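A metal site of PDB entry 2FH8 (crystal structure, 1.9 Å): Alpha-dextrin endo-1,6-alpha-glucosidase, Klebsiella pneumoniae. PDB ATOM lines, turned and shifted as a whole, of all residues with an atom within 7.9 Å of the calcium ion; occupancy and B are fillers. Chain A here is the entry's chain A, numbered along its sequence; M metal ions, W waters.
Four residues have an atom within 4 Å of the calcium ion: Ala 550, Asp 553, Tyr 555 and Asp 893. The nearest printed residue that does not touch the calcium ion is Asn 556 (4.5 Å).
The calcium ion is bound by O of Tyr 555 (2.3 Å), OD2 of Asp 893 (2.3 Å), OD1 of Asp 553 (2.4 Å), O of Ala 550 (2.4 Å), water W2 (2.4 Å), water W3 (2.5 Å) and water W1 (2.6 Å). The calcium ion has seven donor atoms within binding distance.
Water W2 bridges the backbone carbonyl oxygen of Asp 553 (2.6 Å) and the backbone carbonyl oxygen of Thr 484 (3.5 Å). Water W1 lies within hydrogen-bond range of the side-chain amide nitrogen (ND2) of Asn 556, the backbone carbonyl oxygen (O) of Thr 484 and the side-chain carboxylate (OD1) of Asp 893. Water W3 lies within hydrogen-bond range of the side-chain carboxylate (OD2) of Asp 553 (2.6 Å), the backbone carbonyl oxygen (O) of Asp 893 (3.1 Å) and the backbone NH (N) of Gly 895 (3.2 Å).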
ATOM      1  N   THR A 484      26.564  18.651 -28.745  1.00  0.00           N
ATOM      2  CA  THR A 484      26.181  20.059 -28.884  1.00  0.00           C
ATOM      3  C   THR A 484      26.870  20.995 -29.878  1.00  0.00           C
ATOM      4  O   THR A 484      26.799  22.219 -29.733  1.00  0.00           O
ATOM      5  CB  THR A 484      26.194  20.738 -27.511  1.00  0.00           C
ATOM      6  OG1 THR A 484      27.422  20.451 -26.846  1.00  0.00           O
ATOM      7  CG2 THR A 484      25.042  20.228 -26.668  1.00  0.00           C
ATOM      8  N   VAL A 485      27.517  20.432 -30.883  1.00  0.00           N
ATOM      9  CA  VAL A 485      28.157  21.219 -31.930  1.00  0.00           C
ATOM     10  C   VAL A 485      27.850  20.438 -33.200  1.00  0.00           C
ATOM     11  O   VAL A 485      28.077  19.232 -33.247  1.00  0.00           O
ATOM     12  CB  VAL A 485      29.676  21.340 -31.749  1.00  0.00           C
ATOM     13  CG1 VAL A 485      30.312  21.905 -33.022  1.00  0.00           C
ATOM     14  CG2 VAL A 485      29.997  22.265 -30.571  1.00  0.00           C
ATOM     15  N   ASN A 486      27.293  21.098 -34.202  1.00  0.00           N
ATOM     16  CA  ASN A 486      26.986  20.407 -35.447  1.00  0.00           C
ATOM     17  C   ASN A 486      28.304  20.263 -36.191  1.00  0.00           C
ATOM     18  O   ASN A 486      29.042  21.237 -36.378  1.00  0.00           O
ATOM     19  CB  ASN A 486      26.001  21.225 -36.284  1.00  0.00           C
ATOM     20  CG  ASN A 486      25.434  20.432 -37.444  1.00  0.00           C
ATOM     21  OD1 ASN A 486      26.171  19.766 -38.171  1.00  0.00           O
ATOM     22  ND2 ASN A 486      24.116  20.486 -37.606  1.00  0.00           N
ATOM     23  N   ASP A 494      30.672  30.980 -37.370  1.00  0.00           N
ATOM     24  CA  ASP A 494      31.470  31.476 -36.264  1.00  0.00           C
ATOM     25  C   ASP A 494      31.651  32.985 -36.371  1.00  0.00           C
ATOM     26  O   ASP A 494      31.398  33.569 -37.429  1.00  0.00           O
ATOM     27  CB  ASP A 494      32.819  30.747 -36.226  1.00  0.00           C
ATOM     28  CG  ASP A 494      32.687  29.332 -35.676  1.00  0.00           C
ATOM     29  OD1 ASP A 494      32.369  29.197 -34.468  1.00  0.00           O
ATOM     30  OD2 ASP A 494      32.901  28.366 -36.431  1.00  0.00           O
ATOM     31  N   ASN A 546      25.347  37.601 -28.927  1.00  0.00           N
ATOM     32  CA  ASN A 546      26.148  36.401 -28.727  1.00  0.00           C
ATOM     33  C   ASN A 546      25.325  35.186 -28.316  1.00  0.00           C
ATOM     34  O   ASN A 546      25.686  34.057 -28.633  1.00  0.00           O
ATOM     35  CB  ASN A 546      27.236  36.654 -27.687  1.00  0.00           C
ATOM     36  CG  ASN A 546      28.319  35.601 -27.712  1.00  0.00           C
ATOM     37  OD1 ASN A 546      28.946  35.386 -28.756  1.00  0.00           O
ATOM     38  ND2 ASN A 546      28.546  34.940 -26.582  1.00  0.00           N
ATOM     39  N   THR A 547      24.218  35.413 -27.619  1.00  0.00           N
ATOM     40  CA  THR A 547      23.373  34.305 -27.181  1.00  0.00           C
ATOM     41  C   THR A 547      22.740  33.604 -28.372  1.00  0.00           C
ATOM     42  O   THR A 547      22.500  32.398 -28.333  1.00  0.00           O
ATOM     43  CB  THR A 547      22.268  34.780 -26.221  1.00  0.00           C
ATOM     44  OG1 THR A 547      22.874  35.248 -25.008  1.00  0.00           O
ATOM     45  CG2 THR A 547      21.301  33.656 -25.900  1.00  0.00           C
ATOM     46  N   LEU A 548      22.467  34.349 -29.437  1.00  0.00           N
ATOM     47  CA  LEU A 548      21.890  33.779 -30.645  1.00  0.00           C
ATOM     48  C   LEU A 548      23.013  33.098 -31.418  1.00  0.00           C
ATOM     49  O   LEU A 548      22.834  32.017 -31.983  1.00  0.00           O
ATOM     50  CB  LEU A 548      21.245  34.875 -31.495  1.00  0.00           C
ATOM     51  CG  LEU A 548      20.192  35.697 -30.752  1.00  0.00           C
ATOM     52  CD1 LEU A 548      19.644  36.818 -31.631  1.00  0.00           C
ATOM     53  CD2 LEU A 548      19.075  34.770 -30.298  1.00  0.00           C
ATOM     54  N   VAL A 549      24.181  33.738 -31.427  1.00  0.00           N
ATOM     55  CA  VAL A 549      25.356  33.191 -32.102  1.00  0.00           C
ATOM     56  C   VAL A 549      25.710  31.803 -31.563  1.00  0.00           C
ATOM     57  O   VAL A 549      25.989  30.874 -32.323  1.00  0.00           O
ATOM     58  CB  VAL A 549      26.597  34.110 -31.903  1.00  0.00           C
ATOM     59  CG1 VAL A 549      27.854  33.422 -32.438  1.00  0.00           C
ATOM     60  CG2 VAL A 549      26.382  35.454 -32.606  1.00  0.00           C
ATOM     61  N   ALA A 550      25.684  31.684 -30.241  1.00  0.00           N
ATOM     62  CA  ALA A 550      26.023  30.433 -29.556  1.00  0.00           C
ATOM     63  C   ALA A 550      25.207  29.214 -30.015  1.00  0.00           C
ATOM     64  O   ALA A 550      25.673  28.085 -29.879  1.00  0.00           O
ATOM     65  CB  ALA A 550      25.873  30.619 -28.051  1.00  0.00           C
ATOM     66  N   GLN A 551      24.016  29.452 -30.556  1.00  0.00           N
ATOM     67  CA  GLN A 551      23.169  28.353 -31.004  1.00  0.00           C
ATOM     68  C   GLN A 551      23.731  27.600 -32.212  1.00  0.00           C
ATOM     69  O   GLN A 551      23.515  26.400 -32.355  1.00  0.00           O
ATOM     70  CB  GLN A 551      21.781  28.885 -31.367  1.00  0.00           C
ATOM     71  CG  GLN A 551      21.020  29.553 -30.233  1.00  0.00           C
ATOM     72  CD  GLN A 551      19.789  30.300 -30.716  1.00  0.00           C
ATOM     73  OE1 GLN A 551      19.012  30.825 -29.924  1.00  0.00           O
ATOM     74  NE2 GLN A 551      19.626  30.360 -32.029  1.00  0.00           N
ATOM     75  N   THR A 552      24.453  28.308 -33.077  1.00  0.00           N
ATOM     76  CA  THR A 552      24.979  27.693 -34.281  1.00  0.00           C
ATOM     77  C   THR A 552      26.475  27.838 -34.549  1.00  0.00           C
ATOM     78  O   THR A 552      26.915  27.658 -35.679  1.00  0.00           O
ATOM     79  CB  THR A 552      24.199  28.210 -35.527  1.00  0.00           C
ATOM     80  OG1 THR A 552      24.263  29.639 -35.562  1.00  0.00           O
ATOM     81  CG2 THR A 552      22.746  27.785 -35.464  1.00  0.00           C
ATOM     82  N   ASP A 553      27.249  28.149 -33.515  1.00  0.00           N
ATOM     83  CA  ASP A 553      28.695  28.288 -33.688  1.00  0.00           C
ATOM     84  C   ASP A 553      29.395  26.959 -33.409  1.00  0.00           C
ATOM     85  O   ASP A 553      28.739  25.938 -33.201  1.00  0.00           O
ATOM     86  CB  ASP A 553      29.262  29.400 -32.777  1.00  0.00           C
ATOM     87  CG  ASP A 553      29.068  29.115 -31.293  1.00  0.00           C
ATOM     88  OD1 ASP A 553      28.713  27.976 -30.924  1.00  0.00           O
ATOM     89  OD2 ASP A 553      29.309  30.048 -30.484  1.00  0.00           O
ATOM     90  N   SER A 554      30.720  26.968 -33.416  1.00  0.00           N
ATOM     91  CA  SER A 554      31.490  25.758 -33.167  1.00  0.00           C
ATOM     92  C   SER A 554      31.881  25.628 -31.694  1.00  0.00           C
ATOM     93  O   SER A 554      32.680  24.753 -31.337  1.00  0.00           O
ATOM     94  CB  SER A 554      32.759  25.770 -34.014  1.00  0.00           C
ATOM     95  OG  SER A 554      32.467  25.947 -35.389  1.00  0.00           O
ATOM     96  N   TYR A 555      31.325  26.477 -30.840  1.00  0.00           N
ATOM     97  CA  TYR A 555      31.718  26.449 -29.440  1.00  0.00           C
ATOM     98  C   TYR A 555      30.814  25.785 -28.386  1.00  0.00           C
ATOM     99  O   TYR A 555      29.608  25.993 -28.339  1.00  0.00           O
ATOM    100  CB  TYR A 555      32.035  27.870 -28.981  1.00  0.00           C
ATOM    101  CG  TYR A 555      32.792  27.920 -27.684  1.00  0.00           C
ATOM    102  CD1 TYR A 555      32.163  27.660 -26.464  1.00  0.00           C
ATOM    103  CD2 TYR A 555      34.168  28.154 -27.670  1.00  0.00           C
ATOM    104  CE1 TYR A 555      32.886  27.621 -25.275  1.00  0.00           C
ATOM    105  CE2 TYR A 555      34.897  28.124 -26.489  1.00  0.00           C
ATOM    106  CZ  TYR A 555      34.255  27.851 -25.293  1.00  0.00           C
ATOM    107  OH  TYR A 555      34.983  27.776 -24.137  1.00  0.00           O
ATOM    108  N   ASN A 556      31.449  24.988 -27.538  1.00  0.00           N
ATOM    109  CA  ASN A 556      30.789  24.330 -26.415  1.00  0.00           C
ATOM    110  C   ASN A 556      31.838  23.563 -25.604  1.00  0.00           C
ATOM    111  O   ASN A 556      32.745  22.951 -26.186  1.00  0.00           O
ATOM    112  CB  ASN A 556      29.713  23.359 -26.916  1.00  0.00           C
ATOM    113  CG  ASN A 556      28.696  23.031 -25.843  1.00  0.00           C
ATOM    114  OD1 ASN A 556      28.997  22.346 -24.867  1.00  0.00           O
ATOM    115  ND2 ASN A 556      27.481  23.553 -26.000  1.00  0.00           N
ATOM    116  N   TRP A 557      31.746  23.626 -24.288  1.00  0.00           N
ATOM    117  CA  TRP A 557      32.701  22.896 -23.436  1.00  0.00           C
ATOM    118  C   TRP A 557      32.648  21.425 -23.816  1.00  0.00           C
ATOM    119  O   TRP A 557      33.658  20.723 -23.789  1.00  0.00           O
ATOM    120  CB  TRP A 557      32.363  23.028 -21.963  1.00  0.00           C
ATOM    121  CG  TRP A 557      32.773  24.316 -21.325  1.00  0.00           C
ATOM    122  CD1 TRP A 557      33.567  25.288 -21.861  1.00  0.00           C
ATOM    123  CD2 TRP A 557      32.384  24.773 -20.027  1.00  0.00           C
ATOM    124  NE1 TRP A 557      33.704  26.321 -20.965  1.00  0.00           N
ATOM    125  CE2 TRP A 557      32.982  26.033 -19.831  1.00  0.00           C
ATOM    126  CE3 TRP A 557      31.586  24.237 -19.002  1.00  0.00           C
ATOM    127  CZ2 TRP A 557      32.811  26.774 -18.663  1.00  0.00           C
ATOM    128  CZ3 TRP A 557      31.414  24.978 -17.834  1.00  0.00           C
ATOM    129  CH2 TRP A 557      32.024  26.234 -17.680  1.00  0.00           C
ATOM    130  N   TYR A 892      30.073  27.782 -20.577  1.00  0.00           N
ATOM    131  CA  TYR A 892      30.008  26.594 -21.435  1.00  0.00           C
ATOM    132  C   TYR A 892      29.480  26.797 -22.863  1.00  0.00           C
ATOM    133  O   TYR A 892      29.805  26.013 -23.758  1.00  0.00           O
ATOM    134  CB  TYR A 892      29.156  25.499 -20.784  1.00  0.00           C
ATOM    135  CG  TYR A 892      27.660  25.674 -20.970  1.00  0.00           C
ATOM    136  CD1 TYR A 892      26.954  26.649 -20.274  1.00  0.00           C
ATOM    137  CD2 TYR A 892      26.953  24.867 -21.868  1.00  0.00           C
ATOM    138  CE1 TYR A 892      25.583  26.809 -20.443  1.00  0.00           C
ATOM    139  CE2 TYR A 892      25.574  25.018 -22.052  1.00  0.00           C
ATOM    140  CZ  TYR A 892      24.903  25.989 -21.335  1.00  0.00           C
ATOM    141  OH  TYR A 892      23.535  26.127 -21.480  1.00  0.00           O
ATOM    142  N   ASP A 893      28.658  27.809 -23.070  1.00  0.00           N
ATOM    143  CA  ASP A 893      28.106  28.050 -24.394  1.00  0.00           C
ATOM    144  C   ASP A 893      28.160  29.534 -24.711  1.00  0.00           C
ATOM    145  O   ASP A 893      27.341  30.048 -25.473  1.00  0.00           O
ATOM    146  CB  ASP A 893      26.642  27.545 -24.458  1.00  0.00           C
ATOM    147  CG  ASP A 893      26.181  27.266 -25.872  1.00  0.00           C
ATOM    148  OD1 ASP A 893      24.960  27.069 -26.080  1.00  0.00           O
ATOM    149  OD2 ASP A 893      27.036  27.227 -26.784  1.00  0.00           O
ATOM    150  N   SER A 894      29.125  30.224 -24.115  1.00  0.00           N
ATOM    151  CA  SER A 894      29.276  31.661 -24.342  1.00  0.00           C
ATOM    152  C   SER A 894      30.215  32.001 -25.495  1.00  0.00           C
ATOM    153  O   SER A 894      30.675  33.141 -25.615  1.00  0.00           O
ATOM    154  CB  SER A 894      29.726  32.334 -23.049  1.00  0.00           C
ATOM    155  OG  SER A 894      28.745  32.200 -22.044  1.00  0.00           O
ATOM    156  N   GLY A 895      30.507  30.992 -26.318  1.00  0.00           N
ATOM    157  CA  GLY A 895      31.346  31.159 -27.495  1.00  0.00           C
ATOM    158  C   GLY A 895      32.755  31.694 -27.406  1.00  0.00           C
ATOM    159  O   GLY A 895      33.321  31.870 -26.320  1.00  0.00           O
ATOM    160  N   ASP A 896      33.342  31.952 -28.576  1.00  0.00           N
ATOM    161  CA  ASP A 896      34.708  32.473 -28.647  1.00  0.00           C
ATOM    162  C   ASP A 896      34.830  33.824 -27.967  1.00  0.00           C
ATOM    163  O   ASP A 896      35.879  34.141 -27.404  1.00  0.00           O
ATOM    164  CB  ASP A 896      35.156  32.644 -30.113  1.00  0.00           C
ATOM    165  CG  ASP A 896      35.288  31.327 -30.849  1.00  0.00           C
ATOM    166  OD1 ASP A 896      35.635  30.300 -30.222  1.00  0.00           O
ATOM    167  OD2 ASP A 896      35.069  31.327 -32.084  1.00  0.00           O
HETATM  168 CA    CA M   1      27.634  26.963 -29.010  1.00  0.00          CA
HETATM  169  O   HOH W   1      26.236  24.908 -28.362  1.00  0.00           O
HETATM  170  O   HOH W   2      27.652  25.410 -30.888  1.00  0.00           O
HETATM  171  O   HOH W   3      28.595  29.105 -28.120  1.00  0.00           O
